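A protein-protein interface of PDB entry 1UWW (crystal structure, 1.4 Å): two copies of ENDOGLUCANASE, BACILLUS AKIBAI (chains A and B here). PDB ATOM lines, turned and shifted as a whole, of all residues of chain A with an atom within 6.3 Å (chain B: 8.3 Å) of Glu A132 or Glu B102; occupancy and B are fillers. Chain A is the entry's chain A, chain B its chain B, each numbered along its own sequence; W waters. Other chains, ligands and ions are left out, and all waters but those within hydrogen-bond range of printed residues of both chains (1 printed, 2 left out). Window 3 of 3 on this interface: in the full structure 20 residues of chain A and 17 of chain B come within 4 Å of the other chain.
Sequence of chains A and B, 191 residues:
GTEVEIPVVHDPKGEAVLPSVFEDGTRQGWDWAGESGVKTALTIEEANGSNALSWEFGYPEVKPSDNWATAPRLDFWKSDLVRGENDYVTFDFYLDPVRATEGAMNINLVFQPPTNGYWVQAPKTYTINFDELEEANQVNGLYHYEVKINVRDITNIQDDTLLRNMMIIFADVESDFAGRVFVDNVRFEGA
OE2 of Glu B132 lies close to OD2 of Asp A131 (2.6 Å).
ND2 of Asn A129 is in hydrogen-bond range of OD1 of Asn B129 (3.1 Å).
The side-chain carboxylate (OE2) of Glu A132 is in hydrogen-bond range of the backbone NH (N) of Gly B103 (3.0 Å).
The side-chain amide nitrogen of Asn B129 sits at hydrogen-bond distance from the side-chain carboxylate of Asp A131 (3.3 Å).
The backbone carbonyl oxygen (O) of Gly B103 lies within hydrogen-bond range of the side-chain amide nitrogen (ND2) of Asn A129 (3.5 Å).
The backbone NH of Gly A103 is in hydrogen-bond range of the side-chain carboxylate of Glu B132, 2.8 Å away.
The side-chain amide nitrogen (ND2) of Asn A129 is in hydrogen-bond range of the side-chain carboxylate (OD2) of Asp B131 (3.3 Å).
OE2 of Glu A132 lies close to OD2 of Asp B131, at 2.5 Å.
OD1 of Asn B129 is in hydrogen-bond range of N of Asp B131 (3.0 Å).
The backbone carbonyl oxygen (O) of Gly A103 lies within hydrogen-bond range of the backbone NH (N) of Phe A130 (2.9 Å).
N of Asp A131 lies within hydrogen-bond range of OD1 of Asn A129, at 3.0 Å.
The side-chain carboxylate (OD1) of Asp B176 lies within hydrogen-bond range of the backbone NH (N) of Glu B102.
O of Gly B103 sits at hydrogen-bond distance from N of Phe B130.
Gly A103 touches Asn B129 (O to ND2, 3.6 Å).
Asp B131 touches Asp A131 (CB to CB, 3.5 Å).
OE2 of Glu A132 touches CB of Glu B102, at 3.4 Å.
Of the printed residues of chain B, Gly A103 touches Asn B129 and Glu B132.
Of the printed residues of chain B, Asn A129 touches Gly B103 (3.5 Å), Asn B129 (3.1 Å) and Asp B131 (3.3 Å).
Glu A132 touches just these residues of chain B: Glu B102 (3.4 Å), Gly B103 (3.0 Å) and Asp B131 (2.5 Å).
Glu A134 touches none of the printed residues of chain B.
Glu A135 touches none of the printed residues of chain B.
Glu B102 touches one residue of chain A.
Printed residues of chain A within 4 Å of Asn B129: Gly A103, Asn A129 and Asp A131.
Of the printed residues of chain A, Asp B131 touches Asn A129, Asp A131 and Glu A132.
The nearest residue of chain B that does not touch Glu A132 is Thr B101 (4.8 Å).
The nearest residue of chain A that does not touch Glu B102 is Asn A129 (5.6 Å).
The nearest printed residue of chain A that does not touch Asn B129 is Phe A130 (5.3 Å).
Among the printed residues, 11 pairs touch across the chains.
Among the printed residues, no Asp or Glu carboxylate lies within 4 Å of a Lys or Arg side-chain nitrogen of the other chain.
Gly A103 touches Asn B129, and with the chains exchanged Asn A129 touches Gly B103.
Asn B129 touches its own counterpart, Asn A129.
Asn A129 touches Asp B131, and with the chains exchanged Asp A131 touches Asn B129.
Asp A131 touches its own counterpart, Asp B131.
Positions printed for both chains: 103, 129, 130, 131, 132 and 133.
Of the 11 pairs that touch across the chains among the printed residues, 10 have their exchanged pair printed and touching as well.
Water W1 lies within hydrogen-bond range of the backbone carbonyl oxygen of Val B173 (3.1 Å), the side-chain amide nitrogen of Asn A129 (3.1 Å) and the backbone NH of Ala B104 (3.4 Å).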
ATOM      1  N   GLY A 103     -23.027   5.273  -2.305  1.00  0.00           N
ATOM      2  CA  GLY A 103     -22.432   6.347  -1.566  1.00  0.00           C
ATOM      3  C   GLY A 103     -22.708   6.310  -0.074  1.00  0.00           C
ATOM      4  O   GLY A 103     -23.004   5.283   0.526  1.00  0.00           O
ATOM      5  N   ASN A 129     -23.221   4.665   5.623  1.00  0.00           N
ATOM      6  CA  ASN A 129     -22.845   4.059   4.350  1.00  0.00           C
ATOM      7  C   ASN A 129     -24.088   3.435   3.709  1.00  0.00           C
ATOM      8  O   ASN A 129     -24.647   2.459   4.222  1.00  0.00           O
ATOM      9  CB  ASN A 129     -21.755   3.017   4.601  1.00  0.00           C
ATOM     10  CG  ASN A 129     -21.102   2.540   3.340  1.00  0.00           C
ATOM     11  OD1 ASN A 129     -21.731   2.511   2.277  1.00  0.00           O
ATOM     12  ND2 ASN A 129     -19.835   2.169   3.435  1.00  0.00           N
ATOM     13  N   PHE A 130     -24.540   3.997   2.589  1.00  0.00           N
ATOM     14  CA  PHE A 130     -25.778   3.500   1.946  1.00  0.00           C
ATOM     15  C   PHE A 130     -25.605   2.122   1.340  1.00  0.00           C
ATOM     16  O   PHE A 130     -26.597   1.436   1.046  1.00  0.00           O
ATOM     17  CB  PHE A 130     -26.310   4.501   0.926  1.00  0.00           C
ATOM     18  CG  PHE A 130     -26.723   5.827   1.543  1.00  0.00           C
ATOM     19  CD1 PHE A 130     -27.714   5.862   2.523  1.00  0.00           C
ATOM     20  CD2 PHE A 130     -26.135   6.997   1.190  1.00  0.00           C
ATOM     21  CE1 PHE A 130     -28.096   7.066   3.107  1.00  0.00           C
ATOM     22  CE2 PHE A 130     -26.528   8.200   1.762  1.00  0.00           C
ATOM     23  CZ  PHE A 130     -27.516   8.217   2.727  1.00  0.00           C
ATOM     24  N   ASP A 131     -24.368   1.671   1.188  1.00  0.00           N
ATOM     25  CA  ASP A 131     -24.148   0.319   0.706  1.00  0.00           C
ATOM     26  C   ASP A 131     -24.322  -0.704   1.795  1.00  0.00           C
ATOM     27  O   ASP A 131     -24.310  -1.914   1.520  1.00  0.00           O
ATOM     28  CB  ASP A 131     -22.748   0.180   0.117  1.00  0.00           C
ATOM     29  CG  ASP A 131     -22.558   1.035  -1.089  1.00  0.00           C
ATOM     30  OD1 ASP A 131     -23.484   1.088  -1.948  1.00  0.00           O
ATOM     31  OD2 ASP A 131     -21.540   1.734  -1.245  1.00  0.00           O
ATOM     32  N   GLU A 132     -24.468  -0.241   3.035  1.00  0.00           N
ATOM     33  CA  GLU A 132     -24.602  -1.119   4.182  1.00  0.00           C
ATOM     34  C   GLU A 132     -26.023  -1.073   4.793  1.00  0.00           C
ATOM     35  O   GLU A 132     -26.195  -1.453   5.952  1.00  0.00           O
ATOM     36  CB  GLU A 132     -23.559  -0.753   5.254  1.00  0.00           C
ATOM     37  CG  GLU A 132     -22.111  -0.694   4.767  1.00  0.00           C
ATOM     38  CD  GLU A 132     -21.432  -2.020   4.766  1.00  0.00           C
ATOM     39  OE1 GLU A 132     -22.000  -3.015   5.299  1.00  0.00           O
ATOM     40  OE2 GLU A 132     -20.316  -2.069   4.216  1.00  0.00           O
ATOM     41  N   LEU A 133     -27.032  -0.611   4.055  1.00  0.00           N
ATOM     42  CA  LEU A 133     -28.409  -0.558   4.601  1.00  0.00           C
ATOM     43  C   LEU A 133     -28.996  -1.902   5.055  1.00  0.00           C
ATOM     44  O   LEU A 133     -29.797  -1.968   6.003  1.00  0.00           O
ATOM     45  CB  LEU A 133     -29.354   0.103   3.596  1.00  0.00           C
ATOM     46  CG  LEU A 133     -29.154   1.591   3.359  1.00  0.00           C
ATOM     47  CD1 LEU A 133     -30.065   2.074   2.255  1.00  0.00           C
ATOM     48  CD2 LEU A 133     -29.396   2.377   4.628  1.00  0.00           C
ATOM     49  N   GLU A 134     -28.596  -2.970   4.399  1.00  0.00           N
ATOM     50  CA  GLU A 134     -29.108  -4.303   4.709  1.00  0.00           C
ATOM     51  C   GLU A 134     -28.643  -4.758   6.106  1.00  0.00           C
ATOM     52  O   GLU A 134     -29.299  -5.600   6.727  1.00  0.00           O
ATOM     53  CB  GLU A 134     -28.673  -5.278   3.602  1.00  0.00           C
ATOM     54  CG  GLU A 134     -27.165  -5.335   3.375  1.00  0.00           C
ATOM     55  CD  GLU A 134     -26.618  -4.345   2.338  1.00  0.00           C
ATOM     56  OE1 GLU A 134     -27.285  -3.326   1.990  1.00  0.00           O
ATOM     57  OE2 GLU A 134     -25.487  -4.591   1.867  1.00  0.00           O
ATOM     58  N   GLU A 135     -27.552  -4.170   6.605  1.00  0.00           N
ATOM     59  CA  GLU A 135     -26.994  -4.449   7.944  1.00  0.00           C
ATOM     60  C   GLU A 135     -27.462  -3.478   9.042  1.00  0.00           C
ATOM     61  O   GLU A 135     -27.171  -3.694  10.219  1.00  0.00           O
ATOM     62  CB  GLU A 135     -25.451  -4.417   7.909  1.00  0.00           C
ATOM     63  CG  GLU A 135     -24.777  -5.671   7.350  1.00  0.00           C
ATOM     64  CD  GLU A 135     -24.905  -5.826   5.846  1.00  0.00           C
ATOM     65  OE1 GLU A 135     -24.651  -4.839   5.103  1.00  0.00           O
ATOM     66  OE2 GLU A 135     -25.263  -6.943   5.401  1.00  0.00           O
ATOM     67  N   ALA A 136     -28.141  -2.398   8.657  1.00  0.00           N
ATOM     68  CA  ALA A 136     -28.593  -1.370   9.592  1.00  0.00           C
ATOM     69  C   ALA A 136     -29.850  -1.808  10.318  1.00  0.00           C
ATOM     70  O   ALA A 136     -30.616  -2.616   9.811  1.00  0.00           O
ATOM     71  CB  ALA A 136     -28.868  -0.049   8.840  1.00  0.00           C
ATOM     72  N   TYR A 145     -30.327   5.089  13.109  1.00  0.00           N
ATOM     73  CA  TYR A 145     -28.936   5.263  13.512  1.00  0.00           C
ATOM     74  C   TYR A 145     -28.874   6.024  14.829  1.00  0.00           C
ATOM     75  O   TYR A 145     -29.565   7.004  15.037  1.00  0.00           O
ATOM     76  CB  TYR A 145     -28.162   6.043  12.443  1.00  0.00           C
ATOM     77  CG  TYR A 145     -28.125   5.328  11.146  1.00  0.00           C
ATOM     78  CD1 TYR A 145     -29.163   5.481  10.224  1.00  0.00           C
ATOM     79  CD2 TYR A 145     -27.118   4.414  10.853  1.00  0.00           C
ATOM     80  CE1 TYR A 145     -29.185   4.788   9.035  1.00  0.00           C
ATOM     81  CE2 TYR A 145     -27.151   3.694   9.643  1.00  0.00           C
ATOM     82  CZ  TYR A 145     -28.174   3.895   8.776  1.00  0.00           C
ATOM     83  OH  TYR A 145     -28.172   3.192   7.590  1.00  0.00           O
ATOM     84  N   TYR B  59      -7.444  -2.417  10.835  1.00  0.00           N
ATOM     85  CA  TYR B  59      -8.306  -1.929  11.879  1.00  0.00           C
ATOM     86  C   TYR B  59      -8.921  -3.104  12.647  1.00  0.00           C
ATOM     87  O   TYR B  59      -9.540  -3.960  12.022  1.00  0.00           O
ATOM     88  CB  TYR B  59      -9.444  -1.149  11.246  1.00  0.00           C
ATOM     89  CG  TYR B  59      -9.079   0.173  10.593  1.00  0.00           C
ATOM     90  CD1 TYR B  59      -8.472   1.186  11.309  1.00  0.00           C
ATOM     91  CD2 TYR B  59      -9.399   0.418   9.264  1.00  0.00           C
ATOM     92  CE1 TYR B  59      -8.189   2.420  10.698  1.00  0.00           C
ATOM     93  CE2 TYR B  59      -9.132   1.635   8.670  1.00  0.00           C
ATOM     94  CZ  TYR B  59      -8.532   2.615   9.386  1.00  0.00           C
ATOM     95  OH  TYR B  59      -8.268   3.836   8.783  1.00  0.00           O
ATOM     96  N   ARG B  99      -7.556  -7.504   3.005  1.00  0.00           N
ATOM     97  CA  ARG B  99      -9.000  -7.603   3.226  1.00  0.00           C
ATOM     98  C   ARG B  99      -9.579  -6.199   3.145  1.00  0.00           C
ATOM     99  O   ARG B  99      -9.108  -5.302   3.828  1.00  0.00           O
ATOM    100  CB  ARG B  99      -9.294  -8.188   4.603  1.00  0.00           C
ATOM    101  CG  ARG B  99     -10.770  -8.296   4.959  1.00  0.00           C
ATOM    102  CD  ARG B  99     -11.331  -9.703   4.929  1.00  0.00           C
ATOM    103  NE  ARG B  99     -12.792  -9.660   4.802  1.00  0.00           N
ATOM    104  CZ  ARG B  99     -13.554 -10.657   4.363  1.00  0.00           C
ATOM    105  NH1 ARG B  99     -13.036 -11.828   4.079  1.00  0.00           N
ATOM    106  NH2 ARG B  99     -14.861 -10.495   4.251  1.00  0.00           N
ATOM    107  N   ALA B 100     -10.626  -6.027   2.352  1.00  0.00           N
ATOM    108  CA  ALA B 100     -11.375  -4.773   2.300  1.00  0.00           C
ATOM    109  C   ALA B 100     -12.707  -5.066   1.603  1.00  0.00           C
ATOM    110  O   ALA B 100     -12.773  -5.148   0.380  1.00  0.00           O
ATOM    111  CB  ALA B 100     -10.584  -3.697   1.550  1.00  0.00           C
ATOM    112  N   THR B 101     -13.741  -5.324   2.386  1.00  0.00           N
ATOM    113  CA  THR B 101     -15.048  -5.702   1.830  1.00  0.00           C
ATOM    114  C   THR B 101     -16.203  -4.952   2.423  1.00  0.00           C
ATOM    115  O   THR B 101     -17.327  -5.148   1.984  1.00  0.00           O
ATOM    116  CB  THR B 101     -15.330  -7.199   2.050  1.00  0.00           C
ATOM    117  OG1 THR B 101     -15.579  -7.484   3.438  1.00  0.00           O
ATOM    118  CG2 THR B 101     -14.138  -8.093   1.604  1.00  0.00           C
ATOM    119  N   GLU B 102     -15.958  -4.146   3.443  1.00  0.00           N
ATOM    120  CA  GLU B 102     -17.060  -3.412   4.028  1.00  0.00           C
ATOM    121  C   GLU B 102     -16.567  -2.151   4.683  1.00  0.00           C
ATOM    122  O   GLU B 102     -15.375  -1.978   4.962  1.00  0.00           O
ATOM    123  CB  GLU B 102     -17.820  -4.284   5.030  1.00  0.00           C
ATOM    124  CG  GLU B 102     -17.000  -4.736   6.216  1.00  0.00           C
ATOM    125  CD  GLU B 102     -17.699  -5.785   7.089  1.00  0.00           C
ATOM    126  OE1 GLU B 102     -18.688  -6.404   6.636  1.00  0.00           O
ATOM    127  OE2 GLU B 102     -17.240  -6.015   8.224  1.00  0.00           O
ATOM    128  N   GLY B 103     -17.508  -1.250   4.904  1.00  0.00           N
ATOM    129  CA  GLY B 103     -17.217   0.001   5.565  1.00  0.00           C
ATOM    130  C   GLY B 103     -16.481   1.003   4.704  1.00  0.00           C
ATOM    131  O   GLY B 103     -16.557   1.014   3.468  1.00  0.00           O
ATOM    132  N   ALA B 104     -15.835   1.922   5.405  1.00  0.00           N
ATOM    133  CA  ALA B 104     -15.203   3.084   4.772  1.00  0.00           C
ATOM    134  C   ALA B 104     -14.029   3.561   5.617  1.00  0.00           C
ATOM    135  O   ALA B 104     -13.788   3.073   6.716  1.00  0.00           O
ATOM    136  CB  ALA B 104     -16.247   4.237   4.571  1.00  0.00           C
ATOM    137  N   MET B 105     -13.304   4.537   5.087  1.00  0.00           N
ATOM    138  CA  MET B 105     -12.211   5.214   5.754  1.00  0.00           C
ATOM    139  C   MET B 105     -12.356   6.717   5.549  1.00  0.00           C
ATOM    140  O   MET B 105     -12.575   7.169   4.432  1.00  0.00           O
ATOM    141  CB  MET B 105     -10.881   4.772   5.147  1.00  0.00           C
ATOM    142  CG  MET B 105      -9.641   5.559   5.617  1.00  0.00           C
ATOM    143  SD  MET B 105      -7.970   5.048   4.694  1.00  0.00           S
ATOM    144  CE  MET B 105      -7.955   3.957   5.649  1.00  0.00           C
ATOM    145  N   ILE B 128     -13.323   7.353   1.648  1.00  0.00           N
ATOM    146  CA  ILE B 128     -13.168   6.220   0.745  1.00  0.00           C
ATOM    147  C   ILE B 128     -14.132   5.115   1.200  1.00  0.00           C
ATOM    148  O   ILE B 128     -14.120   4.703   2.336  1.00  0.00           O
ATOM    149  CB  ILE B 128     -11.718   5.715   0.807  1.00  0.00           C
ATOM    150  CG1 ILE B 128     -10.769   6.804   0.268  1.00  0.00           C
ATOM    151  CG2 ILE B 128     -11.574   4.386   0.056  1.00  0.00           C
ATOM    152  CD1 ILE B 128      -9.313   6.488   0.406  1.00  0.00           C
ATOM    153  N   ASN B 129     -14.980   4.669   0.293  1.00  0.00           N
ATOM    154  CA  ASN B 129     -16.021   3.702   0.597  1.00  0.00           C
ATOM    155  C   ASN B 129     -15.578   2.334   0.066  1.00  0.00           C
ATOM    156  O   ASN B 129     -15.462   2.154  -1.140  1.00  0.00           O
ATOM    157  CB  ASN B 129     -17.330   4.127  -0.085  1.00  0.00           C
ATOM    158  CG  ASN B 129     -18.523   3.322   0.388  1.00  0.00           C
ATOM    159  OD1 ASN B 129     -18.405   2.146   0.707  1.00  0.00           O
ATOM    160  ND2 ASN B 129     -19.708   3.943   0.394  1.00  0.00           N
ATOM    161  N   PHE B 130     -15.327   1.401   0.967  1.00  0.00           N
ATOM    162  CA  PHE B 130     -14.787   0.100   0.565  1.00  0.00           C
ATOM    163  C   PHE B 130     -15.802  -0.754  -0.163  1.00  0.00           C
ATOM    164  O   PHE B 130     -15.433  -1.722  -0.812  1.00  0.00           O
ATOM    165  CB  PHE B 130     -14.171  -0.642   1.758  1.00  0.00           C
ATOM    166  CG  PHE B 130     -12.957   0.035   2.311  1.00  0.00           C
ATOM    167  CD1 PHE B 130     -11.870   0.313   1.499  1.00  0.00           C
ATOM    168  CD2 PHE B 130     -12.900   0.446   3.624  1.00  0.00           C
ATOM    169  CE1 PHE B 130     -10.749   0.939   2.006  1.00  0.00           C
ATOM    170  CE2 PHE B 130     -11.783   1.091   4.106  1.00  0.00           C
ATOM    171  CZ  PHE B 130     -10.717   1.317   3.295  1.00  0.00           C
ATOM    172  N   ASP B 131     -17.083  -0.425  -0.060  1.00  0.00           N
ATOM    173  CA  ASP B 131     -18.096  -1.147  -0.819  1.00  0.00           C
ATOM    174  C   ASP B 131     -18.109  -0.731  -2.272  1.00  0.00           C
ATOM    175  O   ASP B 131     -18.867  -1.308  -3.075  1.00  0.00           O
ATOM    176  CB  ASP B 131     -19.478  -0.905  -0.231  1.00  0.00           C
ATOM    177  CG  ASP B 131     -19.628  -1.491   1.127  1.00  0.00           C
ATOM    178  OD1 ASP B 131     -19.295  -2.683   1.322  1.00  0.00           O
ATOM    179  OD2 ASP B 131     -20.065  -0.830   2.080  1.00  0.00           O
ATOM    180  N   GLU B 132     -17.304   0.268  -2.640  1.00  0.00           N
ATOM    181  CA  GLU B 132     -17.257   0.761  -3.994  1.00  0.00           C
ATOM    182  C   GLU B 132     -15.868   0.681  -4.608  1.00  0.00           C
ATOM    183  O   GLU B 132     -15.540   1.436  -5.517  1.00  0.00           O
ATOM    184  CB  GLU B 132     -17.829   2.162  -4.026  1.00  0.00           C
ATOM    185  CG  GLU B 132     -19.257   2.091  -3.503  1.00  0.00           C
ATOM    186  CD  GLU B 132     -20.054   3.343  -3.670  1.00  0.00           C
ATOM    187  OE1 GLU B 132     -19.551   4.347  -4.196  1.00  0.00           O
ATOM    188  OE2 GLU B 132     -21.236   3.280  -3.267  1.00  0.00           O
ATOM    189  N   LEU B 133     -15.092  -0.301  -4.166  1.00  0.00           N
ATOM    190  CA  LEU B 133     -13.759  -0.521  -4.742  1.00  0.00           C
ATOM    191  C   LEU B 133     -13.756  -0.893  -6.226  1.00  0.00           C
ATOM    192  O   LEU B 133     -12.827  -0.503  -6.926  1.00  0.00           O
ATOM    193  CB  LEU B 133     -12.994  -1.588  -3.969  1.00  0.00           C
ATOM    194  CG  LEU B 133     -12.528  -1.140  -2.591  1.00  0.00           C
ATOM    195  CD1 LEU B 133     -11.986  -2.364  -1.864  1.00  0.00           C
ATOM    196  CD2 LEU B 133     -11.472  -0.054  -2.690  1.00  0.00           C
ATOM    197  N   ASP B 172     -11.079   4.706  10.698  1.00  0.00           N
ATOM    198  CA  ASP B 172     -12.005   3.625  10.400  1.00  0.00           C
ATOM    199  C   ASP B 172     -13.457   4.079  10.451  1.00  0.00           C
ATOM    200  O   ASP B 172     -13.866   4.753  11.399  1.00  0.00           O
ATOM    201  CB  ASP B 172     -11.785   2.510  11.454  1.00  0.00           C
ATOM    202  CG  ASP B 172     -12.466   1.203  11.123  1.00  0.00           C
ATOM    203  OD1 ASP B 172     -12.869   0.944   9.971  1.00  0.00           O
ATOM    204  OD2 ASP B 172     -12.598   0.360  12.050  1.00  0.00           O
ATOM    205  N   VAL B 173     -14.240   3.642   9.486  1.00  0.00           N
ATOM    206  CA  VAL B 173     -15.709   3.711   9.558  1.00  0.00           C
ATOM    207  C   VAL B 173     -16.299   2.305   9.369  1.00  0.00           C
ATOM    208  O   VAL B 173     -16.702   1.925   8.274  1.00  0.00           O
ATOM    209  CB  VAL B 173     -16.281   4.657   8.475  1.00  0.00           C
ATOM    210  CG1 VAL B 173     -17.774   4.846   8.666  1.00  0.00           C
ATOM    211  CG2 VAL B 173     -15.570   6.001   8.458  1.00  0.00           C
ATOM    212  N   GLU B 174     -16.307   1.533  10.445  1.00  0.00           N
ATOM    213  CA  GLU B 174     -16.898   0.195  10.454  1.00  0.00           C
ATOM    214  C   GLU B 174     -16.364  -0.669   9.313  1.00  0.00           C
ATOM    215  O   GLU B 174     -17.097  -1.417   8.684  1.00  0.00           O
ATOM    216  CB  GLU B 174     -18.433   0.276  10.408  1.00  0.00           C
ATOM    217  CG  GLU B 174     -19.059   1.039  11.575  1.00  0.00           C
ATOM    218  CD  GLU B 174     -20.576   0.956  11.598  1.00  0.00           C
ATOM    219  OE1 GLU B 174     -21.208   0.870  10.515  1.00  0.00           O
ATOM    220  OE2 GLU B 174     -21.151   0.978  12.707  1.00  0.00           O
ATOM    221  N   SER B 175     -15.068  -0.566   9.058  1.00  0.00           N
ATOM    222  CA  SER B 175     -14.444  -1.307   7.974  1.00  0.00           C
ATOM    223  C   SER B 175     -13.757  -2.558   8.492  1.00  0.00           C
ATOM    224  O   SER B 175     -13.564  -2.740   9.689  1.00  0.00           O
ATOM    225  CB  SER B 175     -13.446  -0.434   7.211  1.00  0.00           C
ATOM    226  OG  SER B 175     -12.145  -0.485   7.764  1.00  0.00           O
ATOM    227  N   ASP B 176     -13.409  -3.409   7.547  1.00  0.00           N
ATOM    228  CA  ASP B 176     -12.544  -4.544   7.817  1.00  0.00           C
ATOM    229  C   ASP B 176     -11.194  -4.376   7.144  1.00  0.00           C
ATOM    230  O   ASP B 176     -10.481  -5.371   6.955  1.00  0.00           O
ATOM    231  CB  ASP B 176     -13.212  -5.867   7.422  1.00  0.00           C
ATOM    232  CG  ASP B 176     -13.532  -5.973   5.959  1.00  0.00           C
ATOM    233  OD1 ASP B 176     -13.336  -4.992   5.197  1.00  0.00           O
ATOM    234  OD2 ASP B 176     -14.040  -7.040   5.465  1.00  0.00           O
ATOM    235  N   PHE B 177     -10.785  -3.147   6.824  1.00  0.00           N
ATOM    236  CA  PHE B 177      -9.558  -2.935   6.081  1.00  0.00           C
ATOM    237  C   PHE B 177      -8.309  -3.429   6.804  1.00  0.00           C
ATOM    238  O   PHE B 177      -8.090  -3.146   7.969  1.00  0.00           O
ATOM    239  CB  PHE B 177      -9.344  -1.441   5.719  1.00  0.00           C
ATOM    240  CG  PHE B 177      -8.055  -1.223   4.991  1.00  0.00           C
ATOM    241  CD1 PHE B 177      -7.968  -1.471   3.640  1.00  0.00           C
ATOM    242  CD2 PHE B 177      -6.892  -0.921   5.666  1.00  0.00           C
ATOM    243  CE1 PHE B 177      -6.744  -1.337   2.964  1.00  0.00           C
ATOM    244  CE2 PHE B 177      -5.693  -0.800   4.995  1.00  0.00           C
ATOM    245  CZ  PHE B 177      -5.620  -1.009   3.655  1.00  0.00           C
ATOM    246  N   ALA B 178      -7.490  -4.166   6.055  1.00  0.00           N
ATOM    247  CA  ALA B 178      -6.138  -4.518   6.459  1.00  0.00           C
ATOM    248  C   ALA B 178      -5.298  -4.639   5.210  1.00  0.00           C
ATOM    249  O   ALA B 178      -5.722  -5.247   4.219  1.00  0.00           O
ATOM    250  CB  ALA B 178      -6.111  -5.823   7.215  1.00  0.00           C
HETATM  251  O   HOH W   1     -19.051   2.539   6.425  1.00  0.00           O
